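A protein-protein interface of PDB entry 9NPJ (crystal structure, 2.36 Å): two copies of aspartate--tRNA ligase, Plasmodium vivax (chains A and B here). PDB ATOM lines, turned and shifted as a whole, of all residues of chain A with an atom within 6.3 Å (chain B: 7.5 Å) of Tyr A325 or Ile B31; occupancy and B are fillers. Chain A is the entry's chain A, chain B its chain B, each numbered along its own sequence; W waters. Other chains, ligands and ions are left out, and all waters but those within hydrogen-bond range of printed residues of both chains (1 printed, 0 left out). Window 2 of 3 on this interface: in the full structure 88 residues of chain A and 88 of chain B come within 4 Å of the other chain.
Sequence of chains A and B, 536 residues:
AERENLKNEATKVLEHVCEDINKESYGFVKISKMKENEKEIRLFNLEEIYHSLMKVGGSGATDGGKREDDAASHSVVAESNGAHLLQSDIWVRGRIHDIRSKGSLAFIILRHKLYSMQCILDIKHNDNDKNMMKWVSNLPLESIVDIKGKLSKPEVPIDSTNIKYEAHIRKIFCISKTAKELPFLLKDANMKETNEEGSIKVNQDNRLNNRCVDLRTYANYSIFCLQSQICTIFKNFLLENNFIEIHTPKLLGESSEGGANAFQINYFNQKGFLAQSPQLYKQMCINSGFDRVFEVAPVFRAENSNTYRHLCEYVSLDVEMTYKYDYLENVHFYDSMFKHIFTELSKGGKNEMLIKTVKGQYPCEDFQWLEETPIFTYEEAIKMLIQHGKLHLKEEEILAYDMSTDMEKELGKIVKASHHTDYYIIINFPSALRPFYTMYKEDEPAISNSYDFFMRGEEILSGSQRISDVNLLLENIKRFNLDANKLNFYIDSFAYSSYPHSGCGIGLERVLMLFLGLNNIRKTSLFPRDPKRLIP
Hydrophobic or aromatic side chains of chain A that line the printed part of chain B: Tyr A325 and Pro A500. Of the 19 printed residues of chain B, 7 touch a printed residue of chain A. Among the printed residues, 11 pairs touch across the chains. Among the printed residues, no Asp or Glu carboxylate lies within 4 Å of a Lys or Arg side-chain nitrogen of the other chain.
The side-chain hydroxyl (OH) of Tyr A325 is in hydrogen-bond range of the side-chain carboxylate (OD2) of Asp B146 (3.3 Å). NH2 of Arg B93 lies within hydrogen-bond range of O of Lys A324 (3.0 Å). The backbone carbonyl oxygen of Tyr A323 is in hydrogen-bond range of the guanidinium group of Arg B93, 3.4 Å away.
Tyr A325 touches just these residues of chain B: Ile B31, Met B34, Ile B41, Leu B43, Arg B93 and Asp B146. Of chain A, only Tyr A325 (3.0 Å) comes within 4 Å of Ile B31. Of the printed residues of chain A, Arg B93 touches Tyr A323, Lys A324, Tyr A325 and Pro A500. Of the printed residues of chain A, Ile B175 touches Pro A500. Of the printed residues of chain A, Leu B43 touches Lys A324 and Tyr A325. Of the printed residues of chain A, Asp B146 touches Tyr A325 (3.3 Å). Arg B42 touches none of the printed residues of chain A. Ser B176 touches none of the printed residues of chain A. The nearest residue of chain B that does not touch Tyr A325 is Trp B91 (4.9 Å). The nearest residue of chain A that does not touch Ile B31 is Lys A324 (4.04 Å). The nearest printed residue of chain A that does not touch Met B34 is Lys A324 (7.1 Å).
Water W1 bridges NH1 of Arg B93 (3.0 Å) and O of Tyr A323 (3.0 Å).
No position is printed for both chains.
The side-chain carboxylate (OE1) of Glu A329 is in hydrogen-bond range of the backbone NH (N) of Lys A324, 2.9 Å away. The backbone carbonyl oxygen of Pro A500 sits at hydrogen-bond distance from the backbone NH of Tyr A323 (3.1 Å). O of Phe B44 lies within hydrogen-bond range of N of Arg B93 (3.1 Å). OD1 of Asp B146 is in salt-bridge range of NE of Arg B93, 2.6 Å away. The side-chain carboxylate (OE2) of Glu A329 lies within hydrogen-bond range of the backbone NH (N) of Tyr A325 (2.9 Å).
Among the printed residues, pairs that only touch across the chains: Tyr A325 with Ile B31, Tyr A325 with Arg B93, Tyr A325 with Leu B43, Pro A500 with Arg B93, Tyr A325 with Ile B41, Pro A500 with Ile B175, Tyr A325 with Met B34 and Lys A324 with Leu B43.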
ATOM      1  N   TYR A 323      21.176   5.356   9.794  1.00  0.00           N
ATOM      2  CA  TYR A 323      22.269   5.194   8.845  1.00  0.00           C
ATOM      3  C   TYR A 323      22.737   3.733   8.866  1.00  0.00           C
ATOM      4  O   TYR A 323      22.303   2.920   9.692  1.00  0.00           O
ATOM      5  CB  TYR A 323      23.427   6.161   9.151  1.00  0.00           C
ATOM      6  CG  TYR A 323      24.000   6.019  10.541  1.00  0.00           C
ATOM      7  CD1 TYR A 323      25.027   5.101  10.806  1.00  0.00           C
ATOM      8  CD2 TYR A 323      23.520   6.800  11.596  1.00  0.00           C
ATOM      9  CE1 TYR A 323      25.555   4.958  12.094  1.00  0.00           C
ATOM     10  CE2 TYR A 323      24.042   6.682  12.878  1.00  0.00           C
ATOM     11  CZ  TYR A 323      25.059   5.758  13.125  1.00  0.00           C
ATOM     12  OH  TYR A 323      25.568   5.638  14.400  1.00  0.00           O
ATOM     13  N   LYS A 324      23.619   3.386   7.933  1.00  0.00           N
ATOM     14  CA  LYS A 324      24.084   1.997   7.807  1.00  0.00           C
ATOM     15  C   LYS A 324      25.277   1.739   8.713  1.00  0.00           C
ATOM     16  O   LYS A 324      25.181   0.969   9.683  1.00  0.00           O
ATOM     17  CB  LYS A 324      24.415   1.686   6.348  1.00  0.00           C
ATOM     18  CG  LYS A 324      23.243   1.823   5.382  1.00  0.00           C
ATOM     19  CD  LYS A 324      23.734   1.653   3.956  1.00  0.00           C
ATOM     20  CE  LYS A 324      22.778   2.220   2.934  1.00  0.00           C
ATOM     21  NZ  LYS A 324      23.515   2.635   1.694  1.00  0.00           N
ATOM     22  N   TYR A 325      26.419   2.362   8.425  1.00  0.00           N
ATOM     23  CA  TYR A 325      27.594   2.211   9.270  1.00  0.00           C
ATOM     24  C   TYR A 325      28.270   3.523   9.628  1.00  0.00           C
ATOM     25  O   TYR A 325      28.987   3.569  10.635  1.00  0.00           O
ATOM     26  CB  TYR A 325      28.627   1.281   8.608  1.00  0.00           C
ATOM     27  CG  TYR A 325      28.051  -0.046   8.132  1.00  0.00           C
ATOM     28  CD1 TYR A 325      27.817  -1.087   9.024  1.00  0.00           C
ATOM     29  CD2 TYR A 325      27.736  -0.247   6.794  1.00  0.00           C
ATOM     30  CE1 TYR A 325      27.283  -2.301   8.595  1.00  0.00           C
ATOM     31  CE2 TYR A 325      27.200  -1.450   6.356  1.00  0.00           C
ATOM     32  CZ  TYR A 325      26.980  -2.475   7.260  1.00  0.00           C
ATOM     33  OH  TYR A 325      26.448  -3.669   6.825  1.00  0.00           O
ATOM     34  N   ASP A 326      28.059   4.587   8.866  1.00  0.00           N
ATOM     35  CA  ASP A 326      28.719   5.858   9.114  1.00  0.00           C
ATOM     36  C   ASP A 326      27.670   6.961   9.230  1.00  0.00           C
ATOM     37  O   ASP A 326      26.833   7.124   8.335  1.00  0.00           O
ATOM     38  CB  ASP A 326      29.716   6.158   7.991  1.00  0.00           C
ATOM     39  CG  ASP A 326      30.634   7.301   8.328  1.00  0.00           C
ATOM     40  OD1 ASP A 326      30.227   8.151   9.156  1.00  0.00           O
ATOM     41  OD2 ASP A 326      31.755   7.347   7.768  1.00  0.00           O
ATOM     42  N   TYR A 327      27.709   7.718  10.331  1.00  0.00           N
ATOM     43  CA  TYR A 327      26.736   8.799  10.492  1.00  0.00           C
ATOM     44  C   TYR A 327      26.957   9.924   9.487  1.00  0.00           C
ATOM     45  O   TYR A 327      26.043  10.723   9.253  1.00  0.00           O
ATOM     46  CB  TYR A 327      26.758   9.342  11.921  1.00  0.00           C
ATOM     47  CG  TYR A 327      27.792  10.406  12.178  1.00  0.00           C
ATOM     48  CD1 TYR A 327      29.109  10.068  12.489  1.00  0.00           C
ATOM     49  CD2 TYR A 327      27.450  11.760  12.133  1.00  0.00           C
ATOM     50  CE1 TYR A 327      30.067  11.050  12.732  1.00  0.00           C
ATOM     51  CE2 TYR A 327      28.395  12.751  12.380  1.00  0.00           C
ATOM     52  CZ  TYR A 327      29.704  12.391  12.676  1.00  0.00           C
ATOM     53  OH  TYR A 327      30.643  13.371  12.923  1.00  0.00           O
ATOM     54  N   GLU A 329      26.936   9.465   6.422  1.00  0.00           N
ATOM     55  CA  GLU A 329      25.930   9.249   5.378  1.00  0.00           C
ATOM     56  C   GLU A 329      24.780  10.240   5.524  1.00  0.00           C
ATOM     57  O   GLU A 329      24.321  10.828   4.540  1.00  0.00           O
ATOM     58  CB  GLU A 329      25.373   7.824   5.428  1.00  0.00           C
ATOM     59  CG  GLU A 329      26.404   6.712   5.509  1.00  0.00           C
ATOM     60  CD  GLU A 329      25.793   5.411   6.019  1.00  0.00           C
ATOM     61  OE1 GLU A 329      24.561   5.234   5.872  1.00  0.00           O
ATOM     62  OE2 GLU A 329      26.543   4.574   6.581  1.00  0.00           O
ATOM     63  N   PRO A 500      21.199   2.390  14.556  1.00  0.00           N
ATOM     64  CA  PRO A 500      22.049   3.585  14.531  1.00  0.00           C
ATOM     65  C   PRO A 500      21.295   4.704  13.831  1.00  0.00           C
ATOM     66  O   PRO A 500      20.736   4.509  12.749  1.00  0.00           O
ATOM     67  CB  PRO A 500      23.283   3.142  13.732  1.00  0.00           C
ATOM     68  CG  PRO A 500      23.190   1.629  13.663  1.00  0.00           C
ATOM     69  CD  PRO A 500      21.739   1.300  13.732  1.00  0.00           C
ATOM     70  N   VAL B  29      28.979  -7.361  17.307  1.00  0.00           N
ATOM     71  CA  VAL B  29      30.019  -6.556  16.681  1.00  0.00           C
ATOM     72  C   VAL B  29      29.600  -5.096  16.695  1.00  0.00           C
ATOM     73  O   VAL B  29      28.441  -4.763  16.431  1.00  0.00           O
ATOM     74  CB  VAL B  29      30.312  -7.036  15.245  1.00  0.00           C
ATOM     75  CG1 VAL B  29      29.036  -7.063  14.433  1.00  0.00           C
ATOM     76  CG2 VAL B  29      31.354  -6.134  14.598  1.00  0.00           C
ATOM     77  N   LYS B  30      30.560  -4.232  17.011  1.00  0.00           N
ATOM     78  CA  LYS B  30      30.369  -2.795  16.939  1.00  0.00           C
ATOM     79  C   LYS B  30      30.270  -2.344  15.485  1.00  0.00           C
ATOM     80  O   LYS B  30      30.715  -3.032  14.560  1.00  0.00           O
ATOM     81  CB  LYS B  30      31.518  -2.073  17.638  1.00  0.00           C
ATOM     82  CG  LYS B  30      31.640  -2.419  19.108  1.00  0.00           C
ATOM     83  CD  LYS B  30      32.437  -1.361  19.854  1.00  0.00           C
ATOM     84  CE  LYS B  30      32.448  -1.637  21.350  1.00  0.00           C
ATOM     85  NZ  LYS B  30      33.314  -0.677  22.094  1.00  0.00           N
ATOM     86  N   ILE B  31      29.674  -1.164  15.290  1.00  0.00           N
ATOM     87  CA  ILE B  31      29.480  -0.657  13.934  1.00  0.00           C
ATOM     88  C   ILE B  31      30.815  -0.307  13.278  1.00  0.00           C
ATOM     89  O   ILE B  31      30.968  -0.445  12.056  1.00  0.00           O
ATOM     90  CB  ILE B  31      28.516   0.550  13.956  1.00  0.00           C
ATOM     91  CG1 ILE B  31      27.061   0.076  14.025  1.00  0.00           C
ATOM     92  CG2 ILE B  31      28.730   1.439  12.745  1.00  0.00           C
ATOM     93  CD1 ILE B  31      26.680  -0.902  12.939  1.00  0.00           C
ATOM     94  N   SER B  32      31.799   0.139  14.064  1.00  0.00           N
ATOM     95  CA  SER B  32      33.085   0.538  13.497  1.00  0.00           C
ATOM     96  C   SER B  32      33.852  -0.656  12.928  1.00  0.00           C
ATOM     97  O   SER B  32      34.462  -0.554  11.856  1.00  0.00           O
ATOM     98  CB  SER B  32      33.911   1.258  14.560  1.00  0.00           C
ATOM     99  OG  SER B  32      33.766   0.616  15.814  1.00  0.00           O
ATOM    100  N   LYS B  33      33.842  -1.793  13.628  1.00  0.00           N
ATOM    101  CA  LYS B  33      34.480  -3.014  13.129  1.00  0.00           C
ATOM    102  C   LYS B  33      33.511  -3.742  12.192  1.00  0.00           C
ATOM    103  O   LYS B  33      32.971  -4.806  12.499  1.00  0.00           O
ATOM    104  CB  LYS B  33      34.918  -3.907  14.285  1.00  0.00           C
ATOM    105  N   MET B  34      33.304  -3.136  11.008  1.00  0.00           N
ATOM    106  CA  MET B  34      32.357  -3.675  10.033  1.00  0.00           C
ATOM    107  C   MET B  34      32.759  -3.369   8.591  1.00  0.00           C
ATOM    108  O   MET B  34      31.892  -3.296   7.712  1.00  0.00           O
ATOM    109  CB  MET B  34      30.941  -3.136  10.286  1.00  0.00           C
ATOM    110  CG  MET B  34      30.082  -4.010  11.193  1.00  0.00           C
ATOM    111  SD  MET B  34      29.532  -5.519  10.361  1.00  0.00           S
ATOM    112  CE  MET B  34      28.419  -6.218  11.577  1.00  0.00           C
ATOM    113  N   LYS B  35      34.052  -3.188   8.329  1.00  0.00           N
ATOM    114  CA  LYS B  35      34.559  -2.910   6.993  1.00  0.00           C
ATOM    115  C   LYS B  35      35.294  -4.130   6.455  1.00  0.00           C
ATOM    116  O   LYS B  35      35.725  -5.005   7.211  1.00  0.00           O
ATOM    117  CB  LYS B  35      35.490  -1.689   6.998  1.00  0.00           C
ATOM    118  N   GLU B  40      33.533  -1.541   3.245  1.00  0.00           N
ATOM    119  CA  GLU B  40      32.153  -1.443   3.717  1.00  0.00           C
ATOM    120  C   GLU B  40      31.202  -2.280   2.853  1.00  0.00           C
ATOM    121  O   GLU B  40      31.289  -2.276   1.621  1.00  0.00           O
ATOM    122  CB  GLU B  40      31.693   0.021   3.740  1.00  0.00           C
ATOM    123  N   ILE B  41      30.293  -3.000   3.520  1.00  0.00           N
ATOM    124  CA  ILE B  41      29.326  -3.836   2.815  1.00  0.00           C
ATOM    125  C   ILE B  41      28.329  -2.967   2.053  1.00  0.00           C
ATOM    126  O   ILE B  41      28.157  -1.773   2.328  1.00  0.00           O
ATOM    127  CB  ILE B  41      28.601  -4.766   3.801  1.00  0.00           C
ATOM    128  N   ARG B  42      27.648  -3.587   1.085  1.00  0.00           N
ATOM    129  CA  ARG B  42      26.516  -2.968   0.390  1.00  0.00           C
ATOM    130  C   ARG B  42      25.239  -3.481   1.052  1.00  0.00           C
ATOM    131  O   ARG B  42      24.746  -4.564   0.721  1.00  0.00           O
ATOM    132  CB  ARG B  42      26.541  -3.277  -1.103  1.00  0.00           C
ATOM    133  N   LEU B  43      24.698  -2.695   1.984  1.00  0.00           N
ATOM    134  CA  LEU B  43      23.632  -3.155   2.863  1.00  0.00           C
ATOM    135  C   LEU B  43      22.259  -2.866   2.265  1.00  0.00           C
ATOM    136  O   LEU B  43      22.028  -1.798   1.692  1.00  0.00           O
ATOM    137  CB  LEU B  43      23.776  -2.494   4.234  1.00  0.00           C
ATOM    138  CG  LEU B  43      22.928  -2.969   5.411  1.00  0.00           C
ATOM    139  CD1 LEU B  43      23.149  -4.442   5.690  1.00  0.00           C
ATOM    140  CD2 LEU B  43      23.254  -2.130   6.647  1.00  0.00           C
ATOM    141  N   PHE B  44      21.355  -3.834   2.393  1.00  0.00           N
ATOM    142  CA  PHE B  44      19.979  -3.740   1.924  1.00  0.00           C
ATOM    143  C   PHE B  44      19.022  -3.811   3.107  1.00  0.00           C
ATOM    144  O   PHE B  44      19.350  -4.350   4.168  1.00  0.00           O
ATOM    145  CB  PHE B  44      19.619  -4.877   0.945  1.00  0.00           C
ATOM    146  CG  PHE B  44      20.372  -4.838  -0.352  1.00  0.00           C
ATOM    147  CD1 PHE B  44      21.620  -5.438  -0.464  1.00  0.00           C
ATOM    148  CD2 PHE B  44      19.828  -4.221  -1.467  1.00  0.00           C
ATOM    149  CE1 PHE B  44      22.319  -5.407  -1.662  1.00  0.00           C
ATOM    150  CE2 PHE B  44      20.523  -4.187  -2.671  1.00  0.00           C
ATOM    151  CZ  PHE B  44      21.768  -4.781  -2.765  1.00  0.00           C
ATOM    152  N   TRP B  91      23.943  -8.560   1.653  1.00  0.00           N
ATOM    153  CA  TRP B  91      23.810  -8.199   3.061  1.00  0.00           C
ATOM    154  C   TRP B  91      22.464  -7.520   3.304  1.00  0.00           C
ATOM    155  O   TRP B  91      22.003  -6.723   2.480  1.00  0.00           O
ATOM    156  CB  TRP B  91      24.937  -7.262   3.501  1.00  0.00           C
ATOM    157  CG  TRP B  91      26.275  -7.909   3.726  1.00  0.00           C
ATOM    158  CD1 TRP B  91      27.275  -8.067   2.812  1.00  0.00           C
ATOM    159  CD2 TRP B  91      26.778  -8.436   4.963  1.00  0.00           C
ATOM    160  NE1 TRP B  91      28.362  -8.675   3.395  1.00  0.00           N
ATOM    161  CE2 TRP B  91      28.083  -8.912   4.714  1.00  0.00           C
ATOM    162  CE3 TRP B  91      26.248  -8.559   6.252  1.00  0.00           C
ATOM    163  CZ2 TRP B  91      28.867  -9.501   5.709  1.00  0.00           C
ATOM    164  CZ3 TRP B  91      27.027  -9.147   7.239  1.00  0.00           C
ATOM    165  CH2 TRP B  91      28.324  -9.610   6.960  1.00  0.00           C
ATOM    166  N   VAL B  92      21.839  -7.831   4.440  1.00  0.00           N
ATOM    167  CA  VAL B  92      20.525  -7.278   4.765  1.00  0.00           C
ATOM    168  C   VAL B  92      20.395  -7.147   6.279  1.00  0.00           C
ATOM    169  O   VAL B  92      20.730  -8.075   7.025  1.00  0.00           O
ATOM    170  CB  VAL B  92      19.380  -8.142   4.204  1.00  0.00           C
ATOM    171  CG1 VAL B  92      19.151  -9.341   5.094  1.00  0.00           C
ATOM    172  CG2 VAL B  92      18.101  -7.314   4.087  1.00  0.00           C
ATOM    173  N   ARG B  93      19.884  -5.995   6.724  1.00  0.00           N
ATOM    174  CA  ARG B  93      19.684  -5.687   8.132  1.00  0.00           C
ATOM    175  C   ARG B  93      18.202  -5.747   8.478  1.00  0.00           C
ATOM    176  O   ARG B  93      17.344  -5.470   7.639  1.00  0.00           O
ATOM    177  CB  ARG B  93      20.238  -4.302   8.467  1.00  0.00           C
ATOM    178  CG  ARG B  93      19.998  -3.867   9.898  1.00  0.00           C
ATOM    179  CD  ARG B  93      20.687  -2.543  10.187  1.00  0.00           C
ATOM    180  NE  ARG B  93      22.137  -2.653  10.088  1.00  0.00           N
ATOM    181  CZ  ARG B  93      22.974  -1.636  10.230  1.00  0.00           C
ATOM    182  NH1 ARG B  93      22.534  -0.410  10.474  1.00  0.00           N
ATOM    183  NH2 ARG B  93      24.283  -1.851  10.127  1.00  0.00           N
ATOM    184  N   ASP B 146      22.713  -7.965  11.158  1.00  0.00           N
ATOM    185  CA  ASP B 146      23.111  -7.918   9.759  1.00  0.00           C
ATOM    186  C   ASP B 146      23.369  -9.350   9.293  1.00  0.00           C
ATOM    187  O   ASP B 146      24.275 -10.025   9.799  1.00  0.00           O
ATOM    188  CB  ASP B 146      24.350  -7.043   9.565  1.00  0.00           C
ATOM    189  CG  ASP B 146      24.056  -5.557   9.686  1.00  0.00           C
ATOM    190  OD1 ASP B 146      22.882  -5.177   9.920  1.00  0.00           O
ATOM    191  OD2 ASP B 146      25.014  -4.761   9.546  1.00  0.00           O
ATOM    192  N   ILE B 147      22.568  -9.811   8.337  1.00  0.00           N
ATOM    193  CA  ILE B 147      22.623 -11.175   7.829  1.00  0.00           C
ATOM    194  C   ILE B 147      23.193 -11.141   6.418  1.00  0.00           C
ATOM    195  O   ILE B 147      22.790 -10.305   5.603  1.00  0.00           O
ATOM    196  CB  ILE B 147      21.232 -11.831   7.850  1.00  0.00           C
ATOM    197  CG1 ILE B 147      20.843 -12.206   9.284  1.00  0.00           C
ATOM    198  CG2 ILE B 147      21.186 -13.038   6.915  1.00  0.00           C
ATOM    199  CD1 ILE B 147      19.370 -12.535   9.465  1.00  0.00           C
ATOM    200  N   ILE B 175      24.123  -6.234  15.772  1.00  0.00           N
ATOM    201  CA  ILE B 175      24.606  -4.896  16.092  1.00  0.00           C
ATOM    202  C   ILE B 175      23.865  -4.283  17.273  1.00  0.00           C
ATOM    203  O   ILE B 175      24.404  -3.374  17.922  1.00  0.00           O
ATOM    204  CB  ILE B 175      24.508  -3.961  14.879  1.00  0.00           C
ATOM    205  CG1 ILE B 175      23.047  -3.563  14.652  1.00  0.00           C
ATOM    206  CG2 ILE B 175      25.132  -4.636  13.650  1.00  0.00           C
ATOM    207  CD1 ILE B 175      22.861  -2.457  13.642  1.00  0.00           C
ATOM    208  N   SER B 176      22.663  -4.771  17.589  1.00  0.00           N
ATOM    209  CA  SER B 176      21.903  -4.262  18.725  1.00  0.00           C
ATOM    210  C   SER B 176      21.102  -5.391  19.358  1.00  0.00           C
ATOM    211  O   SER B 176      20.195  -5.948  18.725  1.00  0.00           O
ATOM    212  CB  SER B 176      20.977  -3.116  18.300  1.00  0.00           C
ATOM    213  OG  SER B 176      20.454  -2.481  19.450  1.00  0.00           O
HETATM  214  O   HOH W   1      19.984   1.070  10.370  1.00  0.00           O
